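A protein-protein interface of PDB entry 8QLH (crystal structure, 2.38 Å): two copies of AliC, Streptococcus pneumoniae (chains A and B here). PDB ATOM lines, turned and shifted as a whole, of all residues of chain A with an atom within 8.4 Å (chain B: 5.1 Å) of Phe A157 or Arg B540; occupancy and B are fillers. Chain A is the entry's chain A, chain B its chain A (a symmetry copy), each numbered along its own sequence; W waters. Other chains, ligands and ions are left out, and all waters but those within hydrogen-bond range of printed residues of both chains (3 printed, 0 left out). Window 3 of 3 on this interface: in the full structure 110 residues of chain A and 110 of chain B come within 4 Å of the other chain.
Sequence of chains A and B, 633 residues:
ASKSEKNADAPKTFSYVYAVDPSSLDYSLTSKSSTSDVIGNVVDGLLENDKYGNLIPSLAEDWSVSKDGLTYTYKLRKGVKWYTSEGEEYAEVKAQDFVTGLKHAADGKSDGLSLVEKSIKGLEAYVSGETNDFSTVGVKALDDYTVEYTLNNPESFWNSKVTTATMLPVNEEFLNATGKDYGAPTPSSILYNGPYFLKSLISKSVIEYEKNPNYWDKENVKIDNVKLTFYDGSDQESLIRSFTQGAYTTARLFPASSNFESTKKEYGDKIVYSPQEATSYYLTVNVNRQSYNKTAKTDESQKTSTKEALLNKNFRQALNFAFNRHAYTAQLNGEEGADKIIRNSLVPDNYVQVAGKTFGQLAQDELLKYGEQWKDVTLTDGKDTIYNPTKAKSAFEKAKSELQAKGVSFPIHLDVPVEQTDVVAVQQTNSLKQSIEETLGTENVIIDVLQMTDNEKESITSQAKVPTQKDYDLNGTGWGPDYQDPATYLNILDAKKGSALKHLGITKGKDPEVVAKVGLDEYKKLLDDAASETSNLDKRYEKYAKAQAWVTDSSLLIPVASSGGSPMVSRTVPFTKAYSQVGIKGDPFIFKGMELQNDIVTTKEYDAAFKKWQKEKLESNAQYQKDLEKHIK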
ATOM      1  N   LEU A  55     -27.160  11.132  -1.950  1.00  0.00           N
ATOM      2  CA  LEU A  55     -26.124  10.970  -0.937  1.00  0.00           C
ATOM      3  C   LEU A  55     -25.095  12.087  -1.093  1.00  0.00           C
ATOM      4  O   LEU A  55     -24.302  12.088  -2.037  1.00  0.00           O
ATOM      5  CB  LEU A  55     -25.493   9.586  -1.053  1.00  0.00           C
ATOM      6  CG  LEU A  55     -26.461   8.492  -0.602  1.00  0.00           C
ATOM      7  CD1 LEU A  55     -26.117   7.153  -1.214  1.00  0.00           C
ATOM      8  CD2 LEU A  55     -26.486   8.410   0.919  1.00  0.00           C
ATOM      9  N   TYR A  72     -13.125   2.447  -1.765  1.00  0.00           N
ATOM     10  CA  TYR A  72     -13.799   3.716  -1.537  1.00  0.00           C
ATOM     11  C   TYR A  72     -12.996   4.521  -0.530  1.00  0.00           C
ATOM     12  O   TYR A  72     -12.664   4.016   0.547  1.00  0.00           O
ATOM     13  CB  TYR A  72     -15.220   3.502  -1.019  1.00  0.00           C
ATOM     14  CG  TYR A  72     -16.217   3.072  -2.068  1.00  0.00           C
ATOM     15  CD1 TYR A  72     -16.318   1.744  -2.460  1.00  0.00           C
ATOM     16  CD2 TYR A  72     -17.073   3.996  -2.657  1.00  0.00           C
ATOM     17  CE1 TYR A  72     -17.248   1.348  -3.416  1.00  0.00           C
ATOM     18  CE2 TYR A  72     -17.996   3.615  -3.611  1.00  0.00           C
ATOM     19  CZ  TYR A  72     -18.081   2.291  -3.987  1.00  0.00           C
ATOM     20  OH  TYR A  72     -19.000   1.916  -4.940  1.00  0.00           O
ATOM     21  N   LEU A 115     -25.548  -6.089   6.743  1.00  0.00           N
ATOM     22  CA  LEU A 115     -25.509  -5.282   5.529  1.00  0.00           C
ATOM     23  C   LEU A 115     -24.109  -5.258   4.926  1.00  0.00           C
ATOM     24  O   LEU A 115     -23.954  -5.240   3.701  1.00  0.00           O
ATOM     25  CB  LEU A 115     -25.985  -3.861   5.826  1.00  0.00           C
ATOM     26  CG  LEU A 115     -27.365  -3.435   5.323  1.00  0.00           C
ATOM     27  CD1 LEU A 115     -27.450  -1.919   5.240  1.00  0.00           C
ATOM     28  CD2 LEU A 115     -27.683  -4.071   3.975  1.00  0.00           C
ATOM     29  N   VAL A 116     -23.078  -5.256   5.769  1.00  0.00           N
ATOM     30  CA  VAL A 116     -21.703  -5.067   5.326  1.00  0.00           C
ATOM     31  C   VAL A 116     -20.788  -6.211   5.732  1.00  0.00           C
ATOM     32  O   VAL A 116     -19.591  -6.156   5.443  1.00  0.00           O
ATOM     33  CB  VAL A 116     -21.134  -3.730   5.840  1.00  0.00           C
ATOM     34  CG1 VAL A 116     -22.027  -2.568   5.405  1.00  0.00           C
ATOM     35  CG2 VAL A 116     -20.985  -3.766   7.351  1.00  0.00           C
ATOM     36  N   SER A 119     -19.504  -7.752   2.523  1.00  0.00           N
ATOM     37  CA  SER A 119     -19.030  -6.775   1.554  1.00  0.00           C
ATOM     38  C   SER A 119     -17.632  -6.274   1.890  1.00  0.00           C
ATOM     39  O   SER A 119     -16.749  -6.277   1.027  1.00  0.00           O
ATOM     40  CB  SER A 119     -20.009  -5.592   1.476  1.00  0.00           C
ATOM     41  OG  SER A 119     -21.181  -5.936   0.753  1.00  0.00           O
ATOM     42  N   LEU A 151     -13.778  -3.449  -0.592  1.00  0.00           N
ATOM     43  CA  LEU A 151     -14.881  -4.388  -0.712  1.00  0.00           C
ATOM     44  C   LEU A 151     -14.431  -5.650  -1.436  1.00  0.00           C
ATOM     45  O   LEU A 151     -13.422  -5.661  -2.146  1.00  0.00           O
ATOM     46  CB  LEU A 151     -16.059  -3.752  -1.457  1.00  0.00           C
ATOM     47  CG  LEU A 151     -16.573  -2.385  -0.986  1.00  0.00           C
ATOM     48  CD1 LEU A 151     -17.822  -1.976  -1.762  1.00  0.00           C
ATOM     49  CD2 LEU A 151     -16.852  -2.402   0.509  1.00  0.00           C
ATOM     50  N   ASN A 153     -16.445  -7.215  -3.691  1.00  0.00           N
ATOM     51  CA  ASN A 153     -17.001  -7.081  -5.027  1.00  0.00           C
ATOM     52  C   ASN A 153     -17.473  -5.650  -5.224  1.00  0.00           C
ATOM     53  O   ASN A 153     -17.781  -4.958  -4.246  1.00  0.00           O
ATOM     54  CB  ASN A 153     -18.175  -8.048  -5.243  1.00  0.00           C
ATOM     55  CG  ASN A 153     -17.770  -9.492  -5.074  1.00  0.00           C
ATOM     56  OD1 ASN A 153     -17.150 -10.077  -5.960  1.00  0.00           O
ATOM     57  ND2 ASN A 153     -18.108 -10.073  -3.931  1.00  0.00           N
ATOM     58  N   PRO A 154     -17.527  -5.174  -6.467  1.00  0.00           N
ATOM     59  CA  PRO A 154     -18.084  -3.838  -6.711  1.00  0.00           C
ATOM     60  C   PRO A 154     -19.558  -3.788  -6.335  1.00  0.00           C
ATOM     61  O   PRO A 154     -20.312  -4.737  -6.566  1.00  0.00           O
ATOM     62  CB  PRO A 154     -17.876  -3.632  -8.216  1.00  0.00           C
ATOM     63  CG  PRO A 154     -16.805  -4.618  -8.603  1.00  0.00           C
ATOM     64  CD  PRO A 154     -16.993  -5.790  -7.694  1.00  0.00           C
ATOM     65  N   GLU A 155     -19.961  -2.672  -5.728  1.00  0.00           N
ATOM     66  CA  GLU A 155     -21.328  -2.487  -5.241  1.00  0.00           C
ATOM     67  C   GLU A 155     -21.760  -1.066  -5.586  1.00  0.00           C
ATOM     68  O   GLU A 155     -21.400  -0.117  -4.884  1.00  0.00           O
ATOM     69  CB  GLU A 155     -21.419  -2.734  -3.740  1.00  0.00           C
ATOM     70  CG  GLU A 155     -21.281  -4.181  -3.332  1.00  0.00           C
ATOM     71  CD  GLU A 155     -21.734  -4.433  -1.907  1.00  0.00           C
ATOM     72  OE1 GLU A 155     -21.951  -3.454  -1.161  1.00  0.00           O
ATOM     73  OE2 GLU A 155     -21.876  -5.616  -1.535  1.00  0.00           O
ATOM     74  N   SER A 156     -22.548  -0.924  -6.655  1.00  0.00           N
ATOM     75  CA  SER A 156     -23.087   0.384  -7.021  1.00  0.00           C
ATOM     76  C   SER A 156     -23.953   0.991  -5.923  1.00  0.00           C
ATOM     77  O   SER A 156     -24.175   2.207  -5.930  1.00  0.00           O
ATOM     78  CB  SER A 156     -23.897   0.273  -8.313  1.00  0.00           C
ATOM     79  OG  SER A 156     -24.875  -0.750  -8.225  1.00  0.00           O
ATOM     80  N   PHE A 157     -24.439   0.178  -4.986  1.00  0.00           N
ATOM     81  CA  PHE A 157     -25.267   0.626  -3.874  1.00  0.00           C
ATOM     82  C   PHE A 157     -24.488   0.723  -2.569  1.00  0.00           C
ATOM     83  O   PHE A 157     -25.104   0.812  -1.502  1.00  0.00           O
ATOM     84  CB  PHE A 157     -26.457  -0.324  -3.693  1.00  0.00           C
ATOM     85  CG  PHE A 157     -26.073  -1.781  -3.729  1.00  0.00           C
ATOM     86  CD1 PHE A 157     -26.076  -2.485  -4.926  1.00  0.00           C
ATOM     87  CD2 PHE A 157     -25.683  -2.438  -2.571  1.00  0.00           C
ATOM     88  CE1 PHE A 157     -25.713  -3.818  -4.962  1.00  0.00           C
ATOM     89  CE2 PHE A 157     -25.313  -3.768  -2.600  1.00  0.00           C
ATOM     90  CZ  PHE A 157     -25.328  -4.460  -3.797  1.00  0.00           C
ATOM     91  N   TRP A 158     -23.153   0.697  -2.629  1.00  0.00           N
ATOM     92  CA  TRP A 158     -22.352   0.664  -1.408  1.00  0.00           C
ATOM     93  C   TRP A 158     -22.556   1.928  -0.583  1.00  0.00           C
ATOM     94  O   TRP A 158     -22.710   1.865   0.643  1.00  0.00           O
ATOM     95  CB  TRP A 158     -20.866   0.493  -1.733  1.00  0.00           C
ATOM     96  CG  TRP A 158     -20.019   0.949  -0.587  1.00  0.00           C
ATOM     97  CD1 TRP A 158     -19.345   2.132  -0.479  1.00  0.00           C
ATOM     98  CD2 TRP A 158     -19.810   0.256   0.651  1.00  0.00           C
ATOM     99  NE1 TRP A 158     -18.713   2.207   0.740  1.00  0.00           N
ATOM    100  CE2 TRP A 158     -18.983   1.068   1.451  1.00  0.00           C
ATOM    101  CE3 TRP A 158     -20.232  -0.979   1.152  1.00  0.00           C
ATOM    102  CZ2 TRP A 158     -18.566   0.684   2.725  1.00  0.00           C
ATOM    103  CZ3 TRP A 158     -19.819  -1.358   2.421  1.00  0.00           C
ATOM    104  CH2 TRP A 158     -18.995  -0.530   3.190  1.00  0.00           C
ATOM    105  N   ASN A 159     -22.546   3.088  -1.241  1.00  0.00           N
ATOM    106  CA  ASN A 159     -22.669   4.351  -0.522  1.00  0.00           C
ATOM    107  C   ASN A 159     -23.997   4.452   0.214  1.00  0.00           C
ATOM    108  O   ASN A 159     -24.088   5.138   1.238  1.00  0.00           O
ATOM    109  CB  ASN A 159     -22.494   5.524  -1.487  1.00  0.00           C
ATOM    110  CG  ASN A 159     -21.043   5.972  -1.598  1.00  0.00           C
ATOM    111  OD1 ASN A 159     -20.223   5.666  -0.736  1.00  0.00           O
ATOM    112  ND2 ASN A 159     -20.724   6.699  -2.661  1.00  0.00           N
ATOM    113  N   SER A 160     -25.031   3.763  -0.273  1.00  0.00           N
ATOM    114  CA  SER A 160     -26.295   3.724   0.452  1.00  0.00           C
ATOM    115  C   SER A 160     -26.185   3.001   1.787  1.00  0.00           C
ATOM    116  O   SER A 160     -27.088   3.137   2.620  1.00  0.00           O
ATOM    117  CB  SER A 160     -27.377   3.064  -0.405  1.00  0.00           C
ATOM    118  OG  SER A 160     -27.293   1.652  -0.349  1.00  0.00           O
ATOM    119  N   LYS A 161     -25.104   2.251   2.016  1.00  0.00           N
ATOM    120  CA  LYS A 161     -24.915   1.555   3.282  1.00  0.00           C
ATOM    121  C   LYS A 161     -24.158   2.377   4.316  1.00  0.00           C
ATOM    122  O   LYS A 161     -24.211   2.044   5.504  1.00  0.00           O
ATOM    123  CB  LYS A 161     -24.173   0.238   3.059  1.00  0.00           C
ATOM    124  CG  LYS A 161     -24.889  -0.737   2.154  1.00  0.00           C
ATOM    125  CD  LYS A 161     -24.261  -2.111   2.283  1.00  0.00           C
ATOM    126  CE  LYS A 161     -24.577  -2.988   1.094  1.00  0.00           C
ATOM    127  NZ  LYS A 161     -23.825  -4.270   1.178  1.00  0.00           N
ATOM    128  N   VAL A 162     -23.455   3.437   3.904  1.00  0.00           N
ATOM    129  CA  VAL A 162     -22.659   4.210   4.855  1.00  0.00           C
ATOM    130  C   VAL A 162     -23.490   5.151   5.710  1.00  0.00           C
ATOM    131  O   VAL A 162     -22.938   5.782   6.622  1.00  0.00           O
ATOM    132  CB  VAL A 162     -21.562   5.033   4.152  1.00  0.00           C
ATOM    133  CG1 VAL A 162     -20.821   4.178   3.136  1.00  0.00           C
ATOM    134  CG2 VAL A 162     -22.148   6.267   3.496  1.00  0.00           C
ATOM    135  N   THR A 163     -24.795   5.271   5.447  1.00  0.00           N
ATOM    136  CA  THR A 163     -25.690   6.055   6.291  1.00  0.00           C
ATOM    137  C   THR A 163     -26.496   5.186   7.247  1.00  0.00           C
ATOM    138  O   THR A 163     -27.532   5.630   7.753  1.00  0.00           O
ATOM    139  CB  THR A 163     -26.643   6.911   5.449  1.00  0.00           C
ATOM    140  OG1 THR A 163     -27.500   6.064   4.672  1.00  0.00           O
ATOM    141  CG2 THR A 163     -25.859   7.836   4.529  1.00  0.00           C
ATOM    142  N   TYR B 483     -31.116  -1.610   0.941  1.00  0.00           N
ATOM    143  CA  TYR B 483     -30.093  -0.877   0.210  1.00  0.00           C
ATOM    144  C   TYR B 483     -30.695  -0.370  -1.094  1.00  0.00           C
ATOM    145  O   TYR B 483     -31.711  -0.883  -1.573  1.00  0.00           O
ATOM    146  CB  TYR B 483     -28.841  -1.733  -0.043  1.00  0.00           C
ATOM    147  CG  TYR B 483     -29.092  -3.101  -0.656  1.00  0.00           C
ATOM    148  CD1 TYR B 483     -29.388  -4.201   0.139  1.00  0.00           C
ATOM    149  CD2 TYR B 483     -29.010  -3.293  -2.029  1.00  0.00           C
ATOM    150  CE1 TYR B 483     -29.607  -5.450  -0.421  1.00  0.00           C
ATOM    151  CE2 TYR B 483     -29.224  -4.535  -2.594  1.00  0.00           C
ATOM    152  CZ  TYR B 483     -29.522  -5.609  -1.787  1.00  0.00           C
ATOM    153  OH  TYR B 483     -29.738  -6.847  -2.350  1.00  0.00           O
ATOM    154  N   GLN B 484     -30.050   0.652  -1.665  1.00  0.00           N
ATOM    155  CA  GLN B 484     -30.605   1.390  -2.804  1.00  0.00           C
ATOM    156  C   GLN B 484     -30.305   0.654  -4.113  1.00  0.00           C
ATOM    157  O   GLN B 484     -29.536   1.099  -4.968  1.00  0.00           O
ATOM    158  CB  GLN B 484     -30.061   2.811  -2.827  1.00  0.00           C
ATOM    159  CG  GLN B 484     -30.871   3.785  -3.672  1.00  0.00           C
ATOM    160  CD  GLN B 484     -32.204   4.132  -3.045  1.00  0.00           C
ATOM    161  OE1 GLN B 484     -32.272   4.533  -1.882  1.00  0.00           O
ATOM    162  NE2 GLN B 484     -33.274   3.977  -3.812  1.00  0.00           N
ATOM    163  N   ASP B 485     -30.953  -0.504  -4.264  1.00  0.00           N
ATOM    164  CA  ASP B 485     -30.811  -1.338  -5.449  1.00  0.00           C
ATOM    165  C   ASP B 485     -32.073  -2.173  -5.573  1.00  0.00           C
ATOM    166  O   ASP B 485     -32.628  -2.569  -4.540  1.00  0.00           O
ATOM    167  CB  ASP B 485     -29.577  -2.239  -5.343  1.00  0.00           C
ATOM    168  CG  ASP B 485     -29.268  -2.974  -6.634  1.00  0.00           C
ATOM    169  OD1 ASP B 485     -28.728  -2.345  -7.571  1.00  0.00           O
ATOM    170  OD2 ASP B 485     -29.557  -4.188  -6.704  1.00  0.00           O
ATOM    171  N   ALA B 487     -32.388  -5.179  -6.218  1.00  0.00           N
ATOM    172  CA  ALA B 487     -32.181  -6.532  -5.711  1.00  0.00           C
ATOM    173  C   ALA B 487     -32.689  -6.693  -4.284  1.00  0.00           C
ATOM    174  O   ALA B 487     -33.041  -7.807  -3.882  1.00  0.00           O
ATOM    175  CB  ALA B 487     -30.697  -6.905  -5.783  1.00  0.00           C
ATOM    176  N   ALA B 530     -28.779 -10.332 -13.771  1.00  0.00           N
ATOM    177  CA  ALA B 530     -28.804  -8.961 -13.273  1.00  0.00           C
ATOM    178  C   ALA B 530     -27.727  -8.740 -12.218  1.00  0.00           C
ATOM    179  O   ALA B 530     -27.036  -7.713 -12.232  1.00  0.00           O
ATOM    180  CB  ALA B 530     -30.188  -8.628 -12.707  1.00  0.00           C
ATOM    181  N   ALA B 531     -27.572  -9.691 -11.295  1.00  0.00           N
ATOM    182  CA  ALA B 531     -26.556  -9.566 -10.258  1.00  0.00           C
ATOM    183  C   ALA B 531     -25.149  -9.526 -10.827  1.00  0.00           C
ATOM    184  O   ALA B 531     -24.250  -8.975 -10.183  1.00  0.00           O
ATOM    185  CB  ALA B 531     -26.673 -10.719  -9.263  1.00  0.00           C
ATOM    186  N   GLU B 533     -24.050  -7.792 -13.230  1.00  0.00           N
ATOM    187  CA  GLU B 533     -23.679  -6.429 -13.602  1.00  0.00           C
ATOM    188  C   GLU B 533     -23.312  -5.656 -12.339  1.00  0.00           C
ATOM    189  O   GLU B 533     -24.178  -5.184 -11.602  1.00  0.00           O
ATOM    190  CB  GLU B 533     -24.808  -5.756 -14.376  1.00  0.00           C
ATOM    191  CG  GLU B 533     -25.166  -6.453 -15.690  1.00  0.00           C
ATOM    192  CD  GLU B 533     -24.057  -6.364 -16.742  1.00  0.00           C
ATOM    193  OE1 GLU B 533     -23.180  -5.475 -16.638  1.00  0.00           O
ATOM    194  OE2 GLU B 533     -24.061  -7.198 -17.676  1.00  0.00           O
ATOM    195  N   THR B 534     -22.014  -5.530 -12.092  1.00  0.00           N
ATOM    196  CA  THR B 534     -21.472  -4.872 -10.911  1.00  0.00           C
ATOM    197  C   THR B 534     -21.174  -3.386 -11.107  1.00  0.00           C
ATOM    198  O   THR B 534     -21.056  -2.654 -10.115  1.00  0.00           O
ATOM    199  CB  THR B 534     -20.192  -5.584 -10.465  1.00  0.00           C
ATOM    200  OG1 THR B 534     -19.334  -5.820 -11.597  1.00  0.00           O
ATOM    201  CG2 THR B 534     -20.508  -6.915  -9.798  1.00  0.00           C
ATOM    202  N   ASN B 536     -22.038  -1.450 -14.643  1.00  0.00           N
ATOM    203  CA  ASN B 536     -22.930  -0.811 -15.613  1.00  0.00           C
ATOM    204  C   ASN B 536     -24.323  -0.694 -15.005  1.00  0.00           C
ATOM    205  O   ASN B 536     -25.063  -1.677 -14.929  1.00  0.00           O
ATOM    206  CB  ASN B 536     -22.960  -1.612 -16.913  1.00  0.00           C
ATOM    207  CG  ASN B 536     -23.500  -0.818 -18.086  1.00  0.00           C
ATOM    208  OD1 ASN B 536     -24.514  -0.131 -17.971  1.00  0.00           O
ATOM    209  ND2 ASN B 536     -22.820  -0.913 -19.226  1.00  0.00           N
ATOM    210  N   LEU B 537     -24.692   0.517 -14.577  1.00  0.00           N
ATOM    211  CA  LEU B 537     -26.011   0.727 -13.989  1.00  0.00           C
ATOM    212  C   LEU B 537     -27.123   0.567 -15.015  1.00  0.00           C
ATOM    213  O   LEU B 537     -28.219   0.109 -14.667  1.00  0.00           O
ATOM    214  CB  LEU B 537     -26.085   2.110 -13.352  1.00  0.00           C
ATOM    215  CG  LEU B 537     -25.646   2.201 -11.894  1.00  0.00           C
ATOM    216  CD1 LEU B 537     -26.161   3.486 -11.269  1.00  0.00           C
ATOM    217  CD2 LEU B 537     -26.125   0.985 -11.115  1.00  0.00           C
ATOM    218  N   ASP B 538     -26.862   0.936 -16.272  1.00  0.00           N
ATOM    219  CA  ASP B 538     -27.881   0.812 -17.307  1.00  0.00           C
ATOM    220  C   ASP B 538     -28.232  -0.647 -17.552  1.00  0.00           C
ATOM    221  O   ASP B 538     -29.410  -1.019 -17.555  1.00  0.00           O
ATOM    222  CB  ASP B 538     -27.405   1.479 -18.601  1.00  0.00           C
ATOM    223  CG  ASP B 538     -26.837   2.867 -18.371  1.00  0.00           C
ATOM    224  OD1 ASP B 538     -27.479   3.842 -18.815  1.00  0.00           O
ATOM    225  OD2 ASP B 538     -25.743   2.986 -17.775  1.00  0.00           O
ATOM    226  N   LYS B 539     -27.219  -1.489 -17.773  1.00  0.00           N
ATOM    227  CA  LYS B 539     -27.483  -2.910 -17.969  1.00  0.00           C
ATOM    228  C   LYS B 539     -28.029  -3.548 -16.697  1.00  0.00           C
ATOM    229  O   LYS B 539     -28.895  -4.429 -16.759  1.00  0.00           O
ATOM    230  CB  LYS B 539     -26.214  -3.627 -18.431  1.00  0.00           C
ATOM    231  CG  LYS B 539     -25.878  -3.415 -19.899  1.00  0.00           C
ATOM    232  CD  LYS B 539     -24.502  -3.983 -20.238  1.00  0.00           C
ATOM    233  CE  LYS B 539     -24.611  -5.330 -20.936  1.00  0.00           C
ATOM    234  NZ  LYS B 539     -23.457  -6.223 -20.616  1.00  0.00           N
ATOM    235  N   ARG B 540     -27.539  -3.116 -15.534  1.00  0.00           N
ATOM    236  CA  ARG B 540     -27.987  -3.716 -14.281  1.00  0.00           C
ATOM    237  C   ARG B 540     -29.474  -3.477 -14.063  1.00  0.00           C
ATOM    238  O   ARG B 540     -30.238  -4.415 -13.804  1.00  0.00           O
ATOM    239  CB  ARG B 540     -27.181  -3.161 -13.108  1.00  0.00           C
ATOM    240  CG  ARG B 540     -27.557  -3.789 -11.778  1.00  0.00           C
ATOM    241  CD  ARG B 540     -26.789  -3.180 -10.615  1.00  0.00           C
ATOM    242  NE  ARG B 540     -27.207  -3.787  -9.359  1.00  0.00           N
ATOM    243  CZ  ARG B 540     -26.729  -4.934  -8.898  1.00  0.00           C
ATOM    244  NH1 ARG B 540     -25.800  -5.576  -9.586  1.00  0.00           N
ATOM    245  NH2 ARG B 540     -27.169  -5.432  -7.748  1.00  0.00           N
ATOM    246  N   TYR B 541     -29.905  -2.223 -14.181  1.00  0.00           N
ATOM    247  CA  TYR B 541     -31.289  -1.901 -13.865  1.00  0.00           C
ATOM    248  C   TYR B 541     -32.232  -2.378 -14.961  1.00  0.00           C
ATOM    249  O   TYR B 541     -33.388  -2.710 -14.679  1.00  0.00           O
ATOM    250  CB  TYR B 541     -31.431  -0.397 -13.623  1.00  0.00           C
ATOM    251  CG  TYR B 541     -30.739   0.105 -12.363  1.00  0.00           C
ATOM    252  CD1 TYR B 541     -30.238  -0.781 -11.413  1.00  0.00           C
ATOM    253  CD2 TYR B 541     -30.588   1.467 -12.125  1.00  0.00           C
ATOM    254  CE1 TYR B 541     -29.610  -0.320 -10.257  1.00  0.00           C
ATOM    255  CE2 TYR B 541     -29.960   1.935 -10.978  1.00  0.00           C
ATOM    256  CZ  TYR B 541     -29.475   1.035 -10.047  1.00  0.00           C
ATOM    257  OH  TYR B 541     -28.851   1.494  -8.907  1.00  0.00           O
ATOM    258  N   GLU B 542     -31.760  -2.428 -16.208  1.00  0.00           N
ATOM    259  CA  GLU B 542     -32.549  -3.056 -17.262  1.00  0.00           C
ATOM    260  C   GLU B 542     -32.810  -4.520 -16.941  1.00  0.00           C
ATOM    261  O   GLU B 542     -33.946  -4.998 -17.054  1.00  0.00           O
ATOM    262  CB  GLU B 542     -31.839  -2.923 -18.608  1.00  0.00           C
ATOM    263  CG  GLU B 542     -32.003  -1.563 -19.287  1.00  0.00           C
ATOM    264  CD  GLU B 542     -30.940  -1.316 -20.350  1.00  0.00           C
ATOM    265  OE1 GLU B 542     -30.231  -2.277 -20.725  1.00  0.00           O
ATOM    266  OE2 GLU B 542     -30.819  -0.162 -20.815  1.00  0.00           O
ATOM    267  N   LYS B 543     -31.774  -5.240 -16.496  1.00  0.00           N
ATOM    268  CA  LYS B 543     -31.928  -6.665 -16.228  1.00  0.00           C
ATOM    269  C   LYS B 543     -32.773  -6.933 -14.987  1.00  0.00           C
ATOM    270  O   LYS B 543     -33.512  -7.921 -14.957  1.00  0.00           O
ATOM    271  CB  LYS B 543     -30.553  -7.323 -16.107  1.00  0.00           C
ATOM    272  CG  LYS B 543     -29.856  -7.479 -17.453  1.00  0.00           C
ATOM    273  CD  LYS B 543     -28.533  -8.201 -17.323  1.00  0.00           C
ATOM    274  CE  LYS B 543     -27.928  -8.491 -18.692  1.00  0.00           C
ATOM    275  NZ  LYS B 543     -26.453  -8.748 -18.608  1.00  0.00           N
ATOM    276  N   TYR B 544     -32.686  -6.089 -13.953  1.00  0.00           N
ATOM    277  CA  TYR B 544     -33.590  -6.270 -12.819  1.00  0.00           C
ATOM    278  C   TYR B 544     -35.021  -5.904 -13.188  1.00  0.00           C
ATOM    279  O   TYR B 544     -35.964  -6.482 -12.641  1.00  0.00           O
ATOM    280  CB  TYR B 544     -33.127  -5.455 -11.607  1.00  0.00           C
ATOM    281  CG  TYR B 544     -32.100  -6.178 -10.760  1.00  0.00           C
ATOM    282  CD1 TYR B 544     -32.386  -7.414 -10.182  1.00  0.00           C
ATOM    283  CD2 TYR B 544     -30.840  -5.631 -10.543  1.00  0.00           C
ATOM    284  CE1 TYR B 544     -31.434  -8.090  -9.419  1.00  0.00           C
ATOM    285  CE2 TYR B 544     -29.896  -6.288  -9.782  1.00  0.00           C
ATOM    286  CZ  TYR B 544     -30.192  -7.515  -9.221  1.00  0.00           C
ATOM    287  OH  TYR B 544     -29.229  -8.153  -8.463  1.00  0.00           O
ATOM    288  N   ALA B 545     -35.207  -4.961 -14.115  1.00  0.00           N
ATOM    289  CA  ALA B 545     -36.556  -4.655 -14.578  1.00  0.00           C
ATOM    290  C   ALA B 545     -37.180  -5.854 -15.271  1.00  0.00           C
ATOM    291  O   ALA B 545     -38.399  -6.052 -15.193  1.00  0.00           O
ATOM    292  CB  ALA B 545     -36.537  -3.447 -15.511  1.00  0.00           C
HETATM  293  O   HOH W   1     -23.657  -3.275  -8.379  1.00  0.00           O
HETATM  294  O   HOH W   2     -27.424  -0.052  -7.328  1.00  0.00           O
HETATM  295  O   HOH W   3     -23.389  -5.390  -7.268  1.00  0.00           O
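The backbone NH of Gln B484 lies within hydrogen-bond range of the side-chain hydroxyl of Ser A160 (3.2 Å).
O of Phe A157 lies within hydrogen-bond range of OG of Ser A160, at 2.6 Å. The side-chain carboxylate (OD2) of Asp B485 lies within hydrogen-bond range of the backbone NH (N) of Ala B487, at 3.0 Å. The side-chain carboxylate of Asp B485 lies within salt-bridge range of the guanidinium group of Arg B540 (2.8 Å). O of Glu B533 is in hydrogen-bond range of NH1 of Arg B540 (2.6 Å). The guanidinium group of Arg B540 is in hydrogen-bond range of the side-chain hydroxyl of Tyr B544 (3.5 Å).
Thr B534 touches Pro A154 (CB to CB, 3.8 Å). Leu B537 touches Ser A156. CD of Arg B540 touches OG of Ser A156 (3.9 Å). Phe A157 touches Tyr B483 (CD2 to CD2, 3.5 Å). Phe A157 touches Gln B484 (CB to O, 3.6 Å). Asp B485 touches Phe A157. Arg B540 touches Phe A157 (NH2 to CE1, 3.5 Å). Ser A160 touches Tyr B483.
Tyr A72 touches none of the printed residues of chain B. Of chain B, only Tyr B483 (3.5 Å), Gln B484 (3.6 Å), Asp B485 (3.5 Å) and Arg B540 (3.5 Å) come within 4 Å of Phe A157. Asn A159 touches none of the printed residues of chain B. Printed residues of chain A within 4 Å of Gln B484: Phe A157 (3.6 Å) and Ser A160 (3.2 Å). Of the printed residues of chain A, Asp B485 touches Phe A157 (3.5 Å). Of the printed residues of chain A, Thr B534 touches Pro A154 (3.8 Å). Of the printed residues of chain A, Arg B540 touches Ser A156 (3.9 Å) and Phe A157 (3.5 Å). The nearest residue of chain A that does not touch Arg B540 is Pro A154 (6.3 Å). The nearest printed residue of chain A that does not touch Thr B534 is Ser A156 (4.1 Å).
Of the 18 printed residues of chain B, 6 touch a printed residue of chain A. Printed residues of chain B that touch a printed residue of chain A: Tyr B483, Gln B484, Asp B485, Thr B534, Leu B537 and Arg B540. Hydrophobic or aromatic side chains of chain B within 4 Å of the printed part of chain A: Tyr B483 and Leu B537. Hydrophobic or aromatic side chains of chain A within 4 Å of the printed part of chain B: Pro A154 and Phe A157. Among the printed residues, 9 pairs touch across the chains. Among the printed residues, no Asp or Glu carboxylate lies within 4 Å of a Lys or Arg side-chain nitrogen of the other chain.
No position is printed for both chains. Of the 9 pairs that touch across the chains among the printed residues, none has its exchanged pair printed and touching as well.
Water W2 lies within hydrogen-bond range of OH of Tyr B541 (2.6 Å), OD1 of Asp B485 (2.6 Å), OG of Ser A156 (2.8 Å) and O of Gln B484 (3.4 Å). Water W1 lies within hydrogen-bond range of OG of Ser A156 (2.8 Å), O of Thr B534 (3.2 Å) and NH1 of Arg B540 (3.4 Å). Water W3 lies within hydrogen-bond range of the backbone carbonyl oxygen of Pro A154 (3.2 Å) and the guanidinium group of Arg B540 (3.3 Å).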
